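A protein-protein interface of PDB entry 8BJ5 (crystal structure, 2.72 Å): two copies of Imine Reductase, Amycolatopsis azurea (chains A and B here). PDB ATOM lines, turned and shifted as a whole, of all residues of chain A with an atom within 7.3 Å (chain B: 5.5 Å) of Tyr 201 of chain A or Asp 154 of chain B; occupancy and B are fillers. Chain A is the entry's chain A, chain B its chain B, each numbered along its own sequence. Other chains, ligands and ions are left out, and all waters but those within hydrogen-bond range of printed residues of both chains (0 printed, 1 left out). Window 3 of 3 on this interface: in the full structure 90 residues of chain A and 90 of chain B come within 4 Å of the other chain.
OH of Tyr 201 of chain A lies within hydrogen-bond range of OD2 of Asp 154 of chain B (2.6 Å). O of Tyr 201 of chain A lies within hydrogen-bond range of NE2 of Gln 170 of chain B (3.2 Å). The side-chain hydroxyl (OH) of Tyr 130 of chain B is in hydrogen-bond range of the side-chain carboxylate (OD2) of Asp 204 of chain A, at 3.4 Å. ND2 of Asn 205 of chain A is in hydrogen-bond range of O of Gln 170 of chain B, 2.9 Å away.
The side-chain hydroxyl of Tyr 130 of chain B lies within hydrogen-bond range of the side-chain amide nitrogen of Gln 170 of chain B. O of Val 131 of chain B is in hydrogen-bond range of N of Asp 154 of chain B. O of Asp 154 of chain B sits at hydrogen-bond distance from N of Tyr 133 of chain B (3.0 Å). The side-chain carboxylate (OD1) of Asp 154 of chain B lies within salt-bridge range of the guanidinium group (NH1) of Arg 152 of chain B, 2.9 Å away.
Among the printed residues, merely in contact across the chains: Tyr 201 of chain A with Phe 132 of chain B (3.4 Å), Tyr 201 of chain A with Tyr 130 of chain B (3.6 Å), Ala 202 of chain A with Gln 170 of chain B (3.8 Å), Tyr 201 of chain A with Phe 166 of chain B (3.9 Å), Phe 198 of chain A with Phe 166 of chain B (3.96 Å) and Phe 198 of chain A with Gln 170 of chain B (3.997 Å).
Of chain B, only Tyr 130, Phe 132, Asp 154, Phe 166 and Gln 170 come within 4 Å of Tyr 201 of chain A. Asp 154 of chain B touches just one residue of chain A: Tyr 201 (2.6 Å). Of the printed residues of chain B, Asn 205 of chain A touches Gln 170 (2.9 Å). Of the printed residues of chain A, Gln 170 of chain B touches Phe 198, Tyr 201, Ala 202 and Asn 205.
Of the 12 printed residues of chain A, 5 touch a printed residue of chain B. Printed residues of chain A that touch a printed residue of chain B: Phe 198, Tyr 201, Ala 202, Asp 204 and Asn 205. Hydrophobic or aromatic side chains of chain A that line the printed part of chain B: Phe 198 and Tyr 201. Of the 11 printed residues of chain B, 5 touch a printed residue of chain A. Printed residues of chain B that touch a printed residue of chain A: Tyr 130, Phe 132, Asp 154, Phe 166 and Gln 170. Hydrophobic or aromatic side chains of chain B within 4 Å of the printed part of chain A: Tyr 130, Phe 132 and Phe 166. Among the printed residues, 10 pairs touch across the chains. Among the printed residues, no Asp or Glu carboxylate lies within 4 Å of a Lys or Arg side-chain nitrogen of the other chain.
No position is printed for both chains. Of the 10 pairs that touch across the chains among the printed residues, none has its exchanged pair printed and touching as well.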
ATOM      1  N   GLU A 196       6.552 -30.159  -4.422  1.00  0.00           N
ATOM      2  CA  GLU A 196       6.012 -28.814  -4.752  1.00  0.00           C
ATOM      3  C   GLU A 196       7.106 -27.761  -4.515  1.00  0.00           C
ATOM      4  O   GLU A 196       7.036 -26.712  -5.160  1.00  0.00           O
ATOM      5  CB  GLU A 196       4.690 -28.546  -4.021  1.00  0.00           C
ATOM      6  CG  GLU A 196       4.736 -27.411  -3.018  1.00  0.00           C
ATOM      7  CD  GLU A 196       5.131 -27.833  -1.622  1.00  0.00           C
ATOM      8  OE1 GLU A 196       4.543 -28.823  -1.133  1.00  0.00           O
ATOM      9  OE2 GLU A 196       6.021 -27.178  -1.032  1.00  0.00           O
ATOM     10  N   LYS A 197       8.076 -28.026  -3.640  1.00  0.00           N
ATOM     11  CA  LYS A 197       9.187 -27.077  -3.320  1.00  0.00           C
ATOM     12  C   LYS A 197      10.242 -27.104  -4.441  1.00  0.00           C
ATOM     13  O   LYS A 197      10.956 -26.079  -4.622  1.00  0.00           O
ATOM     14  CB  LYS A 197       9.839 -27.425  -1.973  1.00  0.00           C
ATOM     15  CG  LYS A 197       9.981 -26.280  -0.962  1.00  0.00           C
ATOM     16  CD  LYS A 197      11.430 -25.823  -0.640  1.00  0.00           C
ATOM     17  CE  LYS A 197      11.863 -24.542  -1.327  1.00  0.00           C
ATOM     18  NZ  LYS A 197      11.787 -23.361  -0.433  1.00  0.00           N
ATOM     19  N   PHE A 198      10.341 -28.222  -5.172  1.00  0.00           N
ATOM     20  CA  PHE A 198      11.376 -28.459  -6.217  1.00  0.00           C
ATOM     21  C   PHE A 198      10.834 -28.129  -7.615  1.00  0.00           C
ATOM     22  O   PHE A 198      11.605 -27.617  -8.436  1.00  0.00           O
ATOM     23  CB  PHE A 198      11.914 -29.891  -6.160  1.00  0.00           C
ATOM     24  CG  PHE A 198      12.905 -30.207  -7.251  1.00  0.00           C
ATOM     25  CD1 PHE A 198      14.104 -29.512  -7.344  1.00  0.00           C
ATOM     26  CD2 PHE A 198      12.622 -31.154  -8.225  1.00  0.00           C
ATOM     27  CE1 PHE A 198      15.003 -29.776  -8.369  1.00  0.00           C
ATOM     28  CE2 PHE A 198      13.524 -31.419  -9.248  1.00  0.00           C
ATOM     29  CZ  PHE A 198      14.710 -30.727  -9.322  1.00  0.00           C
ATOM     30  N   MET A 199       9.544 -28.390  -7.871  1.00  0.00           N
ATOM     31  CA  MET A 199       8.939 -28.312  -9.226  1.00  0.00           C
ATOM     32  C   MET A 199       9.206 -26.949  -9.849  1.00  0.00           C
ATOM     33  O   MET A 199       9.507 -26.893 -11.033  1.00  0.00           O
ATOM     34  CB  MET A 199       7.437 -28.582  -9.188  1.00  0.00           C
ATOM     35  CG  MET A 199       6.825 -28.662 -10.553  1.00  0.00           C
ATOM     36  SD  MET A 199       5.297 -27.695 -10.679  1.00  0.00           S
ATOM     37  CE  MET A 199       5.966 -26.114 -11.197  1.00  0.00           C
ATOM     38  N   PRO A 200       9.127 -25.809  -9.125  1.00  0.00           N
ATOM     39  CA  PRO A 200       9.320 -24.504  -9.756  1.00  0.00           C
ATOM     40  C   PRO A 200      10.716 -24.354 -10.383  1.00  0.00           C
ATOM     41  O   PRO A 200      10.835 -23.727 -11.416  1.00  0.00           O
ATOM     42  CB  PRO A 200       9.115 -23.501  -8.612  1.00  0.00           C
ATOM     43  CG  PRO A 200       8.333 -24.263  -7.573  1.00  0.00           C
ATOM     44  CD  PRO A 200       8.814 -25.690  -7.702  1.00  0.00           C
ATOM     45  N   TYR A 201      11.723 -24.939  -9.749  1.00  0.00           N
ATOM     46  CA  TYR A 201      13.131 -24.960 -10.233  1.00  0.00           C
ATOM     47  C   TYR A 201      13.237 -25.813 -11.516  1.00  0.00           C
ATOM     48  O   TYR A 201      13.905 -25.410 -12.503  1.00  0.00           O
ATOM     49  CB  TYR A 201      14.039 -25.440  -9.097  1.00  0.00           C
ATOM     50  CG  TYR A 201      14.142 -24.502  -7.917  1.00  0.00           C
ATOM     51  CD1 TYR A 201      14.838 -23.312  -8.026  1.00  0.00           C
ATOM     52  CD2 TYR A 201      13.594 -24.819  -6.681  1.00  0.00           C
ATOM     53  CE1 TYR A 201      14.983 -22.456  -6.942  1.00  0.00           C
ATOM     54  CE2 TYR A 201      13.713 -23.964  -5.593  1.00  0.00           C
ATOM     55  CZ  TYR A 201      14.408 -22.775  -5.725  1.00  0.00           C
ATOM     56  OH  TYR A 201      14.564 -21.937  -4.662  1.00  0.00           O
ATOM     57  N   ALA A 202      12.590 -26.978 -11.533  1.00  0.00           N
ATOM     58  CA  ALA A 202      12.542 -27.878 -12.713  1.00  0.00           C
ATOM     59  C   ALA A 202      11.854 -27.133 -13.868  1.00  0.00           C
ATOM     60  O   ALA A 202      12.407 -27.118 -14.984  1.00  0.00           O
ATOM     61  CB  ALA A 202      11.839 -29.168 -12.353  1.00  0.00           C
ATOM     62  N   LYS A 203      10.717 -26.486 -13.602  1.00  0.00           N
ATOM     63  CA  LYS A 203      10.004 -25.645 -14.595  1.00  0.00           C
ATOM     64  C   LYS A 203      10.990 -24.651 -15.214  1.00  0.00           C
ATOM     65  O   LYS A 203      11.121 -24.652 -16.446  1.00  0.00           O
ATOM     66  CB  LYS A 203       8.807 -24.916 -13.971  1.00  0.00           C
ATOM     67  CG  LYS A 203       7.766 -24.459 -14.979  1.00  0.00           C
ATOM     68  CD  LYS A 203       6.530 -23.848 -14.346  1.00  0.00           C
ATOM     69  CE  LYS A 203       6.009 -22.621 -15.071  1.00  0.00           C
ATOM     70  NZ  LYS A 203       5.153 -22.982 -16.231  1.00  0.00           N
ATOM     71  N   ASP A 204      11.653 -23.829 -14.404  1.00  0.00           N
ATOM     72  CA  ASP A 204      12.641 -22.823 -14.879  1.00  0.00           C
ATOM     73  C   ASP A 204      13.705 -23.556 -15.703  1.00  0.00           C
ATOM     74  O   ASP A 204      13.962 -23.096 -16.828  1.00  0.00           O
ATOM     75  CB  ASP A 204      13.236 -22.033 -13.712  1.00  0.00           C
ATOM     76  CG  ASP A 204      14.492 -21.259 -14.053  1.00  0.00           C
ATOM     77  OD1 ASP A 204      14.350 -20.246 -14.738  1.00  0.00           O
ATOM     78  OD2 ASP A 204      15.604 -21.704 -13.638  1.00  0.00           O
ATOM     79  N   ASN A 205      14.257 -24.671 -15.181  1.00  0.00           N
ATOM     80  CA  ASN A 205      15.317 -25.487 -15.833  1.00  0.00           C
ATOM     81  C   ASN A 205      14.937 -25.750 -17.288  1.00  0.00           C
ATOM     82  O   ASN A 205      15.721 -25.393 -18.168  1.00  0.00           O
ATOM     83  CB  ASN A 205      15.548 -26.806 -15.098  1.00  0.00           C
ATOM     84  CG  ASN A 205      16.798 -27.544 -15.542  1.00  0.00           C
ATOM     85  OD1 ASN A 205      17.200 -27.496 -16.703  1.00  0.00           O
ATOM     86  ND2 ASN A 205      17.413 -28.268 -14.622  1.00  0.00           N
ATOM     87  N   PHE A 206      13.776 -26.360 -17.520  1.00  0.00           N
ATOM     88  CA  PHE A 206      13.265 -26.732 -18.866  1.00  0.00           C
ATOM     89  C   PHE A 206      13.013 -25.469 -19.709  1.00  0.00           C
ATOM     90  O   PHE A 206      13.324 -25.467 -20.913  1.00  0.00           O
ATOM     91  CB  PHE A 206      11.978 -27.555 -18.750  1.00  0.00           C
ATOM     92  CG  PHE A 206      12.137 -28.988 -18.303  1.00  0.00           C
ATOM     93  CD1 PHE A 206      12.809 -29.907 -19.086  1.00  0.00           C
ATOM     94  CD2 PHE A 206      11.561 -29.434 -17.124  1.00  0.00           C
ATOM     95  CE1 PHE A 206      12.933 -31.227 -18.684  1.00  0.00           C
ATOM     96  CE2 PHE A 206      11.683 -30.756 -16.725  1.00  0.00           C
ATOM     97  CZ  PHE A 206      12.366 -31.648 -17.509  1.00  0.00           C
ATOM     98  N   GLU A 207      12.442 -24.424 -19.103  1.00  0.00           N
ATOM     99  CA  GLU A 207      12.014 -23.185 -19.808  1.00  0.00           C
ATOM    100  C   GLU A 207      13.232 -22.389 -20.273  1.00  0.00           C
ATOM    101  O   GLU A 207      13.072 -21.560 -21.194  1.00  0.00           O
ATOM    102  CB  GLU A 207      11.075 -22.370 -18.924  1.00  0.00           C
ATOM    103  CG  GLU A 207       9.642 -22.885 -19.030  1.00  0.00           C
ATOM    104  CD  GLU A 207       8.673 -22.418 -17.965  1.00  0.00           C
ATOM    105  OE1 GLU A 207       8.995 -21.421 -17.272  1.00  0.00           O
ATOM    106  OE2 GLU A 207       7.601 -23.073 -17.827  1.00  0.00           O
ATOM    107  N   TYR B 130      20.613 -17.405  -9.789  1.00  0.00           N
ATOM    108  CA  TYR B 130      20.197 -17.819  -8.431  1.00  0.00           C
ATOM    109  C   TYR B 130      21.150 -18.930  -7.980  1.00  0.00           C
ATOM    110  O   TYR B 130      21.751 -19.627  -8.824  1.00  0.00           O
ATOM    111  CB  TYR B 130      18.721 -18.219  -8.405  1.00  0.00           C
ATOM    112  CG  TYR B 130      18.378 -19.500  -9.122  1.00  0.00           C
ATOM    113  CD1 TYR B 130      18.111 -19.518 -10.482  1.00  0.00           C
ATOM    114  CD2 TYR B 130      18.258 -20.691  -8.436  1.00  0.00           C
ATOM    115  CE1 TYR B 130      17.763 -20.683 -11.148  1.00  0.00           C
ATOM    116  CE2 TYR B 130      17.908 -21.870  -9.085  1.00  0.00           C
ATOM    117  CZ  TYR B 130      17.675 -21.870 -10.448  1.00  0.00           C
ATOM    118  OH  TYR B 130      17.370 -23.030 -11.103  1.00  0.00           O
ATOM    119  N   VAL B 131      21.308 -19.061  -6.671  1.00  0.00           N
ATOM    120  CA  VAL B 131      22.314 -19.961  -6.040  1.00  0.00           C
ATOM    121  C   VAL B 131      21.661 -20.638  -4.833  1.00  0.00           C
ATOM    122  O   VAL B 131      21.235 -19.929  -3.891  1.00  0.00           O
ATOM    123  CB  VAL B 131      23.586 -19.182  -5.647  1.00  0.00           C
ATOM    124  CG1 VAL B 131      24.713 -20.118  -5.234  1.00  0.00           C
ATOM    125  CG2 VAL B 131      24.054 -18.256  -6.760  1.00  0.00           C
ATOM    126  N   PHE B 132      21.557 -21.964  -4.872  1.00  0.00           N
ATOM    127  CA  PHE B 132      21.195 -22.793  -3.699  1.00  0.00           C
ATOM    128  C   PHE B 132      22.280 -22.607  -2.643  1.00  0.00           C
ATOM    129  O   PHE B 132      23.468 -22.623  -3.016  1.00  0.00           O
ATOM    130  CB  PHE B 132      21.059 -24.260  -4.099  1.00  0.00           C
ATOM    131  CG  PHE B 132      19.938 -24.526  -5.069  1.00  0.00           C
ATOM    132  CD1 PHE B 132      18.695 -23.911  -4.930  1.00  0.00           C
ATOM    133  CD2 PHE B 132      20.120 -25.397  -6.125  1.00  0.00           C
ATOM    134  CE1 PHE B 132      17.668 -24.188  -5.813  1.00  0.00           C
ATOM    135  CE2 PHE B 132      19.094 -25.644  -7.025  1.00  0.00           C
ATOM    136  CZ  PHE B 132      17.874 -25.036  -6.875  1.00  0.00           C
ATOM    137  N   TYR B 133      21.880 -22.389  -1.390  1.00  0.00           N
ATOM    138  CA  TYR B 133      22.792 -22.284  -0.221  1.00  0.00           C
ATOM    139  C   TYR B 133      22.214 -23.118   0.921  1.00  0.00           C
ATOM    140  O   TYR B 133      20.967 -23.225   1.010  1.00  0.00           O
ATOM    141  CB  TYR B 133      22.985 -20.825   0.205  1.00  0.00           C
ATOM    142  CG  TYR B 133      23.802 -19.974  -0.736  1.00  0.00           C
ATOM    143  CD1 TYR B 133      25.188 -20.061  -0.783  1.00  0.00           C
ATOM    144  CD2 TYR B 133      23.181 -19.048  -1.562  1.00  0.00           C
ATOM    145  CE1 TYR B 133      25.933 -19.267  -1.641  1.00  0.00           C
ATOM    146  CE2 TYR B 133      23.904 -18.232  -2.414  1.00  0.00           C
ATOM    147  CZ  TYR B 133      25.289 -18.340  -2.455  1.00  0.00           C
ATOM    148  OH  TYR B 133      26.029 -17.557  -3.296  1.00  0.00           O
ATOM    149  N   ARG B 152      20.701 -14.465  -6.995  1.00  0.00           N
ATOM    150  CA  ARG B 152      19.655 -14.485  -5.938  1.00  0.00           C
ATOM    151  C   ARG B 152      19.961 -15.666  -5.014  1.00  0.00           C
ATOM    152  O   ARG B 152      20.043 -16.804  -5.489  1.00  0.00           O
ATOM    153  CB  ARG B 152      18.254 -14.595  -6.550  1.00  0.00           C
ATOM    154  CG  ARG B 152      17.141 -14.786  -5.527  1.00  0.00           C
ATOM    155  CD  ARG B 152      15.768 -14.866  -6.171  1.00  0.00           C
ATOM    156  NE  ARG B 152      15.607 -15.985  -7.106  1.00  0.00           N
ATOM    157  CZ  ARG B 152      14.949 -17.118  -6.862  1.00  0.00           C
ATOM    158  NH1 ARG B 152      14.366 -17.304  -5.691  1.00  0.00           N
ATOM    159  NH2 ARG B 152      14.865 -18.064  -7.790  1.00  0.00           N
ATOM    160  N   PRO B 153      20.209 -15.450  -3.704  1.00  0.00           N
ATOM    161  CA  PRO B 153      20.450 -16.551  -2.774  1.00  0.00           C
ATOM    162  C   PRO B 153      19.116 -17.195  -2.371  1.00  0.00           C
ATOM    163  O   PRO B 153      18.236 -16.488  -1.880  1.00  0.00           O
ATOM    164  CB  PRO B 153      21.137 -15.897  -1.562  1.00  0.00           C
ATOM    165  CG  PRO B 153      21.316 -14.430  -1.934  1.00  0.00           C
ATOM    166  CD  PRO B 153      20.318 -14.151  -3.034  1.00  0.00           C
ATOM    167  N   ASP B 154      18.987 -18.502  -2.631  1.00  0.00           N
ATOM    168  CA  ASP B 154      17.878 -19.357  -2.144  1.00  0.00           C
ATOM    169  C   ASP B 154      18.461 -20.236  -1.038  1.00  0.00           C
ATOM    170  O   ASP B 154      19.081 -21.284  -1.350  1.00  0.00           O
ATOM    171  CB  ASP B 154      17.237 -20.152  -3.278  1.00  0.00           C
ATOM    172  CG  ASP B 154      16.594 -19.267  -4.343  1.00  0.00           C
ATOM    173  OD1 ASP B 154      16.735 -18.010  -4.250  1.00  0.00           O
ATOM    174  OD2 ASP B 154      15.944 -19.834  -5.257  1.00  0.00           O
ATOM    175  N   PHE B 155      18.346 -19.760   0.208  1.00  0.00           N
ATOM    176  CA  PHE B 155      18.755 -20.477   1.434  1.00  0.00           C
ATOM    177  C   PHE B 155      17.697 -21.541   1.710  1.00  0.00           C
ATOM    178  O   PHE B 155      16.522 -21.181   1.881  1.00  0.00           O
ATOM    179  CB  PHE B 155      18.927 -19.527   2.611  1.00  0.00           C
ATOM    180  CG  PHE B 155      19.454 -20.239   3.818  1.00  0.00           C
ATOM    181  CD1 PHE B 155      20.807 -20.536   3.929  1.00  0.00           C
ATOM    182  CD2 PHE B 155      18.595 -20.657   4.819  1.00  0.00           C
ATOM    183  CE1 PHE B 155      21.298 -21.219   5.038  1.00  0.00           C
ATOM    184  CE2 PHE B 155      19.087 -21.347   5.920  1.00  0.00           C
ATOM    185  CZ  PHE B 155      20.435 -21.629   6.031  1.00  0.00           C
ATOM    186  N   LEU B 156      18.100 -22.812   1.697  1.00  0.00           N
ATOM    187  CA  LEU B 156      17.178 -23.979   1.726  1.00  0.00           C
ATOM    188  C   LEU B 156      17.003 -24.475   3.163  1.00  0.00           C
ATOM    189  O   LEU B 156      15.970 -25.109   3.425  1.00  0.00           O
ATOM    190  CB  LEU B 156      17.747 -25.087   0.836  1.00  0.00           C
ATOM    191  CG  LEU B 156      17.823 -24.775  -0.655  1.00  0.00           C
ATOM    192  CD1 LEU B 156      18.531 -25.890  -1.404  1.00  0.00           C
ATOM    193  CD2 LEU B 156      16.445 -24.504  -1.233  1.00  0.00           C
ATOM    194  N   PHE B 166      19.764 -30.175  -4.178  1.00  0.00           N
ATOM    195  CA  PHE B 166      18.994 -29.375  -5.159  1.00  0.00           C
ATOM    196  C   PHE B 166      19.842 -29.153  -6.419  1.00  0.00           C
ATOM    197  O   PHE B 166      19.269 -29.077  -7.514  1.00  0.00           O
ATOM    198  CB  PHE B 166      18.521 -28.065  -4.523  1.00  0.00           C
ATOM    199  CG  PHE B 166      17.131 -28.108  -3.952  1.00  0.00           C
ATOM    200  CD1 PHE B 166      16.865 -28.831  -2.806  1.00  0.00           C
ATOM    201  CD2 PHE B 166      16.087 -27.417  -4.563  1.00  0.00           C
ATOM    202  CE1 PHE B 166      15.576 -28.870  -2.290  1.00  0.00           C
ATOM    203  CE2 PHE B 166      14.804 -27.450  -4.037  1.00  0.00           C
ATOM    204  CZ  PHE B 166      14.551 -28.185  -2.908  1.00  0.00           C
ATOM    205  N   GLN B 170      18.918 -30.560 -10.232  1.00  0.00           N
ATOM    206  CA  GLN B 170      18.808 -29.662 -11.413  1.00  0.00           C
ATOM    207  C   GLN B 170      19.653 -30.230 -12.567  1.00  0.00           C
ATOM    208  O   GLN B 170      19.125 -30.375 -13.710  1.00  0.00           O
ATOM    209  CB  GLN B 170      19.202 -28.250 -10.999  1.00  0.00           C
ATOM    210  CG  GLN B 170      18.101 -27.561 -10.184  1.00  0.00           C
ATOM    211  CD  GLN B 170      16.967 -27.076 -11.058  1.00  0.00           C
ATOM    212  OE1 GLN B 170      16.262 -27.882 -11.661  1.00  0.00           O
ATOM    213  NE2 GLN B 170      16.808 -25.766 -11.153  1.00  0.00           N
